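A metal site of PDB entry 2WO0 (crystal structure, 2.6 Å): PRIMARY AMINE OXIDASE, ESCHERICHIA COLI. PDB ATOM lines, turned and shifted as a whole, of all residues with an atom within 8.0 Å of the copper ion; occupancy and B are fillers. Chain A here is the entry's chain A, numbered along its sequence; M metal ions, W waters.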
ATOM      1  N   VAL A 367     -13.026   1.966 -14.001  1.00  0.00           N
ATOM      2  CA  VAL A 367     -11.874   2.430 -14.722  1.00  0.00           C
ATOM      3  C   VAL A 367     -11.512   3.823 -14.248  1.00  0.00           C
ATOM      4  O   VAL A 367     -12.015   4.827 -14.762  1.00  0.00           O
ATOM      5  CB  VAL A 367     -12.128   2.401 -16.221  1.00  0.00           C
ATOM      6  CG1 VAL A 367     -10.825   2.565 -16.977  1.00  0.00           C
ATOM      7  CG2 VAL A 367     -12.808   1.085 -16.565  1.00  0.00           C
ATOM      8  N   TYR A 369      -8.634   6.906 -13.238  1.00  0.00           N
ATOM      9  CA  TYR A 369      -7.510   7.519 -13.926  1.00  0.00           C
ATOM     10  C   TYR A 369      -6.503   8.173 -12.948  1.00  0.00           C
ATOM     11  O   TYR A 369      -6.841   8.464 -11.811  1.00  0.00           O
ATOM     12  CB  TYR A 369      -8.066   8.514 -14.929  1.00  0.00           C
ATOM     13  CG  TYR A 369      -8.617   7.843 -16.167  1.00  0.00           C
ATOM     14  CD1 TYR A 369      -9.924   7.401 -16.225  1.00  0.00           C
ATOM     15  CD2 TYR A 369      -7.795   7.615 -17.261  1.00  0.00           C
ATOM     16  CE1 TYR A 369     -10.402   6.748 -17.351  1.00  0.00           C
ATOM     17  CE2 TYR A 369      -8.259   6.978 -18.374  1.00  0.00           C
ATOM     18  CZ  TYR A 369      -9.552   6.537 -18.433  1.00  0.00           C
ATOM     19  OH  TYR A 369      -9.954   5.925 -19.614  1.00  0.00           O
ATOM     20  N   ASN A 465     -16.086   5.262 -24.585  1.00  0.00           N
ATOM     21  CA  ASN A 465     -15.042   4.956 -25.540  1.00  0.00           C
ATOM     22  C   ASN A 465     -14.640   3.493 -25.487  1.00  0.00           C
ATOM     23  O   ASN A 465     -13.762   3.068 -26.224  1.00  0.00           O
ATOM     24  CB  ASN A 465     -13.835   5.878 -25.300  1.00  0.00           C
ATOM     25  CG  ASN A 465     -13.448   5.952 -23.844  1.00  0.00           C
ATOM     26  OD1 ASN A 465     -14.317   6.142 -22.999  1.00  0.00           O
ATOM     27  ND2 ASN A 465     -12.181   5.753 -23.536  1.00  0.00           N
ATOM     28  N   TPQ A 466     -14.716   2.605 -24.019  1.00  0.00           N
ATOM     29  CA  TPQ A 466     -14.229   1.241 -23.867  1.00  0.00           C
ATOM     30  CB  TPQ A 466     -13.986   0.811 -22.416  1.00  0.00           C
ATOM     31  C   TPQ A 466     -15.294   0.347 -24.388  1.00  0.00           C
ATOM     32  O   TPQ A 466     -16.485   0.761 -24.259  1.00  0.00           O
ATOM     33  C1  TPQ A 466     -13.553   2.051 -21.686  1.00  0.00           C
ATOM     34  C2  TPQ A 466     -12.125   2.451 -21.683  1.00  0.00           C
ATOM     35  O2  TPQ A 466     -11.179   1.673 -22.331  1.00  0.00           O
ATOM     36  C3  TPQ A 466     -11.739   3.603 -21.021  1.00  0.00           C
ATOM     37  C4  TPQ A 466     -12.697   4.355 -20.376  1.00  0.00           C
ATOM     38  O4  TPQ A 466     -12.309   5.475 -19.725  1.00  0.00           O
ATOM     39  C5  TPQ A 466     -14.131   3.935 -20.387  1.00  0.00           C
ATOM     40  O5  TPQ A 466     -15.095   4.660 -19.758  1.00  0.00           O
ATOM     41  C6  TPQ A 466     -14.517   2.790 -21.042  1.00  0.00           C
ATOM     42  N   TYR A 468     -15.975  -3.710 -23.648  1.00  0.00           N
ATOM     43  CA  TYR A 468     -15.473  -4.797 -22.865  1.00  0.00           C
ATOM     44  C   TYR A 468     -16.117  -6.108 -23.271  1.00  0.00           C
ATOM     45  O   TYR A 468     -17.336  -6.183 -23.557  1.00  0.00           O
ATOM     46  CB  TYR A 468     -15.685  -4.528 -21.405  1.00  0.00           C
ATOM     47  CG  TYR A 468     -15.108  -3.230 -20.888  1.00  0.00           C
ATOM     48  CD1 TYR A 468     -13.751  -3.101 -20.597  1.00  0.00           C
ATOM     49  CD2 TYR A 468     -15.929  -2.136 -20.657  1.00  0.00           C
ATOM     50  CE1 TYR A 468     -13.213  -1.909 -20.087  1.00  0.00           C
ATOM     51  CE2 TYR A 468     -15.424  -0.961 -20.146  1.00  0.00           C
ATOM     52  CZ  TYR A 468     -14.061  -0.826 -19.861  1.00  0.00           C
ATOM     53  OH  TYR A 468     -13.569   0.388 -19.359  1.00  0.00           O
ATOM     54  N   ALA A 486     -10.554  -6.020 -23.137  1.00  0.00           N
ATOM     55  CA  ALA A 486     -10.754  -4.572 -23.256  1.00  0.00           C
ATOM     56  C   ALA A 486     -10.243  -4.028 -24.610  1.00  0.00           C
ATOM     57  O   ALA A 486      -9.149  -4.357 -25.056  1.00  0.00           O
ATOM     58  CB  ALA A 486     -10.093  -3.865 -22.095  1.00  0.00           C
ATOM     59  N   THR A 487     -11.073  -3.262 -25.301  1.00  0.00           N
ATOM     60  CA  THR A 487     -10.674  -2.667 -26.580  1.00  0.00           C
ATOM     61  C   THR A 487     -11.456  -1.390 -26.778  1.00  0.00           C
ATOM     62  O   THR A 487     -12.076  -0.869 -25.850  1.00  0.00           O
ATOM     63  CB  THR A 487     -10.973  -3.610 -27.737  1.00  0.00           C
ATOM     64  OG1 THR A 487     -10.653  -2.998 -28.994  1.00  0.00           O
ATOM     65  CG2 THR A 487     -12.471  -4.076 -27.718  1.00  0.00           C
ATOM     66  N   ILE A 489     -11.372   2.720 -27.796  1.00  0.00           N
ATOM     67  CA  ILE A 489     -10.668   3.990 -28.003  1.00  0.00           C
ATOM     68  C   ILE A 489     -10.247   4.624 -26.674  1.00  0.00           C
ATOM     69  O   ILE A 489     -11.091   4.821 -25.777  1.00  0.00           O
ATOM     70  CB  ILE A 489     -11.643   5.019 -28.636  1.00  0.00           C
ATOM     71  CG1 ILE A 489     -12.507   4.392 -29.738  1.00  0.00           C
ATOM     72  CG2 ILE A 489     -10.872   6.233 -29.184  1.00  0.00           C
ATOM     73  CD1 ILE A 489     -11.856   4.330 -31.074  1.00  0.00           C
ATOM     74  N   GLU A 490      -8.966   4.969 -26.546  1.00  0.00           N
ATOM     75  CA  GLU A 490      -8.494   5.590 -25.302  1.00  0.00           C
ATOM     76  C   GLU A 490      -9.012   7.003 -25.049  1.00  0.00           C
ATOM     77  O   GLU A 490      -9.161   7.803 -25.976  1.00  0.00           O
ATOM     78  CB  GLU A 490      -6.981   5.664 -25.237  1.00  0.00           C
ATOM     79  CG  GLU A 490      -6.303   4.441 -25.695  1.00  0.00           C
ATOM     80  CD  GLU A 490      -5.140   4.118 -24.807  1.00  0.00           C
ATOM     81  OE1 GLU A 490      -5.048   4.790 -23.735  1.00  0.00           O
ATOM     82  OE2 GLU A 490      -4.356   3.188 -25.160  1.00  0.00           O
ATOM     83  N   ALA A 491      -9.257   7.277 -23.778  1.00  0.00           N
ATOM     84  CA  ALA A 491      -9.468   8.627 -23.299  1.00  0.00           C
ATOM     85  C   ALA A 491      -8.109   9.311 -23.385  1.00  0.00           C
ATOM     86  O   ALA A 491      -7.189   8.908 -22.677  1.00  0.00           O
ATOM     87  CB  ALA A 491      -9.952   8.602 -21.872  1.00  0.00           C
ATOM     88  N   THR A 522      -3.700   8.962 -21.091  1.00  0.00           N
ATOM     89  CA  THR A 522      -3.608   8.998 -19.631  1.00  0.00           C
ATOM     90  C   THR A 522      -3.665   7.599 -19.011  1.00  0.00           C
ATOM     91  O   THR A 522      -4.524   6.739 -19.421  1.00  0.00           O
ATOM     92  CB  THR A 522      -4.676   9.917 -18.971  1.00  0.00           C
ATOM     93  OG1 THR A 522      -4.657  11.203 -19.605  1.00  0.00           O
ATOM     94  CG2 THR A 522      -4.379  10.117 -17.503  1.00  0.00           C
ATOM     95  N   THR A 523      -2.749   7.367 -18.063  1.00  0.00           N
ATOM     96  CA  THR A 523      -2.642   6.110 -17.357  1.00  0.00           C
ATOM     97  C   THR A 523      -3.868   5.908 -16.503  1.00  0.00           C
ATOM     98  O   THR A 523      -4.366   6.854 -15.904  1.00  0.00           O
ATOM     99  CB  THR A 523      -1.372   6.065 -16.448  1.00  0.00           C
ATOM    100  OG1 THR A 523      -0.220   6.187 -17.265  1.00  0.00           O
ATOM    101  CG2 THR A 523      -1.282   4.767 -15.658  1.00  0.00           C
ATOM    102  N   HIS A 524      -4.348   4.676 -16.444  1.00  0.00           N
ATOM    103  CA  HIS A 524      -5.466   4.340 -15.595  1.00  0.00           C
ATOM    104  C   HIS A 524      -5.369   2.873 -15.303  1.00  0.00           C
ATOM    105  O   HIS A 524      -4.411   2.219 -15.691  1.00  0.00           O
ATOM    106  CB  HIS A 524      -6.745   4.586 -16.365  1.00  0.00           C
ATOM    107  CG  HIS A 524      -6.720   3.968 -17.718  1.00  0.00           C
ATOM    108  ND1 HIS A 524      -5.854   4.396 -18.707  1.00  0.00           N
ATOM    109  CD2 HIS A 524      -7.388   2.900 -18.241  1.00  0.00           C
ATOM    110  CE1 HIS A 524      -6.018   3.656 -19.782  1.00  0.00           C
ATOM    111  NE2 HIS A 524      -6.936   2.745 -19.529  1.00  0.00           N
ATOM    112  N   GLN A 525      -6.393   2.352 -14.664  1.00  0.00           N
ATOM    113  CA  GLN A 525      -6.518   0.929 -14.405  1.00  0.00           C
ATOM    114  C   GLN A 525      -7.830   0.416 -14.962  1.00  0.00           C
ATOM    115  O   GLN A 525      -8.750   1.203 -15.233  1.00  0.00           O
ATOM    116  CB  GLN A 525      -6.522   0.700 -12.906  1.00  0.00           C
ATOM    117  CG  GLN A 525      -5.251   1.163 -12.229  1.00  0.00           C
ATOM    118  CD  GLN A 525      -5.142   0.612 -10.828  1.00  0.00           C
ATOM    119  OE1 GLN A 525      -5.639   1.221  -9.859  1.00  0.00           O
ATOM    120  NE2 GLN A 525      -4.507  -0.567 -10.705  1.00  0.00           N
ATOM    121  N   HIS A 526      -7.927  -0.898 -15.112  1.00  0.00           N
ATOM    122  CA  HIS A 526      -9.172  -1.551 -15.439  1.00  0.00           C
ATOM    123  C   HIS A 526      -9.391  -2.554 -14.327  1.00  0.00           C
ATOM    124  O   HIS A 526      -8.567  -3.437 -14.130  1.00  0.00           O
ATOM    125  CB  HIS A 526      -9.054  -2.318 -16.739  1.00  0.00           C
ATOM    126  CG  HIS A 526      -8.885  -1.441 -17.925  1.00  0.00           C
ATOM    127  ND1 HIS A 526      -9.942  -0.800 -18.521  1.00  0.00           N
ATOM    128  CD2 HIS A 526      -7.784  -1.081 -18.627  1.00  0.00           C
ATOM    129  CE1 HIS A 526      -9.505  -0.085 -19.552  1.00  0.00           C
ATOM    130  NE2 HIS A 526      -8.195  -0.232 -19.623  1.00  0.00           N
ATOM    131  N   TYR A 528     -12.047  -5.246 -12.783  1.00  0.00           N
ATOM    132  CA  TYR A 528     -13.271  -5.992 -12.916  1.00  0.00           C
ATOM    133  C   TYR A 528     -13.439  -6.815 -11.657  1.00  0.00           C
ATOM    134  O   TYR A 528     -12.465  -7.327 -11.107  1.00  0.00           O
ATOM    135  CB  TYR A 528     -13.159  -6.966 -14.077  1.00  0.00           C
ATOM    136  CG  TYR A 528     -12.561  -6.418 -15.334  1.00  0.00           C
ATOM    137  CD1 TYR A 528     -13.329  -5.681 -16.236  1.00  0.00           C
ATOM    138  CD2 TYR A 528     -11.240  -6.691 -15.661  1.00  0.00           C
ATOM    139  CE1 TYR A 528     -12.794  -5.206 -17.421  1.00  0.00           C
ATOM    140  CE2 TYR A 528     -10.697  -6.213 -16.835  1.00  0.00           C
ATOM    141  CZ  TYR A 528     -11.477  -5.473 -17.712  1.00  0.00           C
ATOM    142  OH  TYR A 528     -10.940  -4.993 -18.873  1.00  0.00           O
ATOM    143  N   HIS A 613      -1.902  -7.202 -20.254  1.00  0.00           N
ATOM    144  CA  HIS A 613      -1.490  -5.884 -19.803  1.00  0.00           C
ATOM    145  C   HIS A 613      -0.819  -6.070 -18.450  1.00  0.00           C
ATOM    146  O   HIS A 613      -1.001  -7.095 -17.798  1.00  0.00           O
ATOM    147  CB  HIS A 613      -2.697  -4.967 -19.628  1.00  0.00           C
ATOM    148  CG  HIS A 613      -2.885  -3.946 -20.709  1.00  0.00           C
ATOM    149  ND1 HIS A 613      -1.900  -3.626 -21.629  1.00  0.00           N
ATOM    150  CD2 HIS A 613      -3.931  -3.124 -20.991  1.00  0.00           C
ATOM    151  CE1 HIS A 613      -2.347  -2.679 -22.440  1.00  0.00           C
ATOM    152  NE2 HIS A 613      -3.576  -2.358 -22.074  1.00  0.00           N
ATOM    153  N   THR A 687      -5.958  -4.460 -14.416  1.00  0.00           N
ATOM    154  CA  THR A 687      -4.731  -4.206 -15.108  1.00  0.00           C
ATOM    155  C   THR A 687      -4.341  -2.759 -14.817  1.00  0.00           C
ATOM    156  O   THR A 687      -5.180  -1.947 -14.429  1.00  0.00           O
ATOM    157  CB  THR A 687      -4.927  -4.377 -16.618  1.00  0.00           C
ATOM    158  OG1 THR A 687      -5.961  -3.481 -17.060  1.00  0.00           O
ATOM    159  CG2 THR A 687      -5.316  -5.832 -16.987  1.00  0.00           C
ATOM    160  N   THR A 688      -3.064  -2.436 -14.980  1.00  0.00           N
ATOM    161  CA  THR A 688      -2.612  -1.046 -15.000  1.00  0.00           C
ATOM    162  C   THR A 688      -2.178  -0.688 -16.409  1.00  0.00           C
ATOM    163  O   THR A 688      -1.239  -1.255 -16.958  1.00  0.00           O
ATOM    164  CB  THR A 688      -1.438  -0.854 -14.078  1.00  0.00           C
ATOM    165  OG1 THR A 688      -1.896  -1.059 -12.753  1.00  0.00           O
ATOM    166  CG2 THR A 688      -0.923   0.546 -14.179  1.00  0.00           C
ATOM    167  N   HIS A 689      -2.888   0.239 -17.006  1.00  0.00           N
ATOM    168  CA  HIS A 689      -2.741   0.415 -18.406  1.00  0.00           C
ATOM    169  C   HIS A 689      -1.817   1.605 -18.657  1.00  0.00           C
ATOM    170  O   HIS A 689      -2.215   2.733 -18.440  1.00  0.00           O
ATOM    171  CB  HIS A 689      -4.111   0.612 -19.056  1.00  0.00           C
ATOM    172  CG  HIS A 689      -4.072   0.715 -20.555  1.00  0.00           C
ATOM    173  ND1 HIS A 689      -5.215   0.751 -21.338  1.00  0.00           N
ATOM    174  CD2 HIS A 689      -3.029   0.814 -21.422  1.00  0.00           C
ATOM    175  CE1 HIS A 689      -4.876   0.849 -22.614  1.00  0.00           C
ATOM    176  NE2 HIS A 689      -3.560   0.903 -22.689  1.00  0.00           N
ATOM    177  N   VAL A 690      -0.578   1.327 -19.094  1.00  0.00           N
ATOM    178  CA  VAL A 690       0.307   2.369 -19.623  1.00  0.00           C
ATOM    179  C   VAL A 690       0.292   2.303 -21.137  1.00  0.00           C
ATOM    180  O   VAL A 690       0.594   1.265 -21.718  1.00  0.00           O
ATOM    181  CB  VAL A 690       1.760   2.205 -19.118  1.00  0.00           C
ATOM    182  CG1 VAL A 690       2.657   3.369 -19.600  1.00  0.00           C
ATOM    183  CG2 VAL A 690       1.779   2.105 -17.607  1.00  0.00           C
ATOM    184  N   ALA A 691      -0.078   3.408 -21.779  1.00  0.00           N
ATOM    185  CA  ALA A 691      -0.418   3.387 -23.203  1.00  0.00           C
ATOM    186  C   ALA A 691       0.776   3.215 -24.147  1.00  0.00           C
ATOM    187  O   ALA A 691       1.927   3.426 -23.743  1.00  0.00           O
ATOM    188  CB  ALA A 691      -1.159   4.629 -23.534  1.00  0.00           C
ATOM    189  N   GLU A 695      -1.661   1.219 -29.770  1.00  0.00           N
ATOM    190  CA  GLU A 695      -3.062   1.191 -29.281  1.00  0.00           C
ATOM    191  C   GLU A 695      -3.885   2.387 -29.781  1.00  0.00           C
ATOM    192  O   GLU A 695      -4.968   2.671 -29.261  1.00  0.00           O
ATOM    193  CB  GLU A 695      -3.088   1.132 -27.740  1.00  0.00           C
ATOM    194  CG  GLU A 695      -2.027   0.208 -27.212  1.00  0.00           C
ATOM    195  CD  GLU A 695      -1.861   0.204 -25.696  1.00  0.00           C
ATOM    196  OE1 GLU A 695      -2.154   1.236 -25.024  1.00  0.00           O
ATOM    197  OE2 GLU A 695      -1.416  -0.860 -25.180  1.00  0.00           O
ATOM    198  N   MET A 699      -7.607   0.413 -29.879  1.00  0.00           N
ATOM    199  CA  MET A 699      -6.789  -0.462 -28.993  1.00  0.00           C
ATOM    200  C   MET A 699      -7.051  -1.926 -29.236  1.00  0.00           C
ATOM    201  O   MET A 699      -8.157  -2.402 -29.028  1.00  0.00           O
ATOM    202  CB  MET A 699      -7.056  -0.137 -27.517  1.00  0.00           C
ATOM    203  CG  MET A 699      -6.192  -0.959 -26.527  1.00  0.00           C
ATOM    204  SD  MET A 699      -6.540  -0.733 -24.741  1.00  0.00           S
ATOM    205  CE  MET A 699      -7.431  -2.253 -24.310  1.00  0.00           C
ATOM    206  N   GLU A 702      -7.149  -6.496 -25.232  1.00  0.00           N
ATOM    207  CA  GLU A 702      -6.234  -7.053 -24.223  1.00  0.00           C
ATOM    208  C   GLU A 702      -6.986  -7.883 -23.182  1.00  0.00           C
ATOM    209  O   GLU A 702      -8.051  -7.483 -22.722  1.00  0.00           O
ATOM    210  CB  GLU A 702      -5.496  -5.936 -23.506  1.00  0.00           C
ATOM    211  CG  GLU A 702      -4.790  -4.995 -24.448  1.00  0.00           C
ATOM    212  CD  GLU A 702      -3.325  -5.335 -24.620  1.00  0.00           C
ATOM    213  OE1 GLU A 702      -2.917  -6.486 -24.372  1.00  0.00           O
ATOM    214  OE2 GLU A 702      -2.568  -4.423 -24.991  1.00  0.00           O
HETATM  215 CU    CU M   1      -7.173   1.082 -20.724  1.00  0.00          CU
HETATM  216  O   HOH W   1      -8.848   2.002 -22.012  1.00  0.00           O
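N of Thr 687 sits at hydrogen-bond distance from O of His 526, at 2.8 Å.
A ring nitrogen (ND1) of His 524 sits at hydrogen-bond distance from the backbone carbonyl oxygen of Thr 522 (2.8 Å).
NE2 of His 613 lies close to NE2 of His 689.
The side-chain carboxylate (OE2) of Glu 490 lies within hydrogen-bond range of a ring nitrogen (NE2) of His 689 (3.5 Å).
A ring nitrogen (NE2) of His 689 sits at hydrogen-bond distance from the side-chain carboxylate (OE1) of Glu 695 (2.7 Å).
Within 4 Å of the copper ion: His 524, His 526 and His 689.
The copper ion is bound by a ring nitrogen (NE2) of His 526 (2.0 Å), a ring nitrogen (NE2) of His 524 (2.1 Å), a ring nitrogen (ND1) of His 689 (2.1 Å) and water W1 (2.3 Å).
The copper ion has four donor atoms within binding distance.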
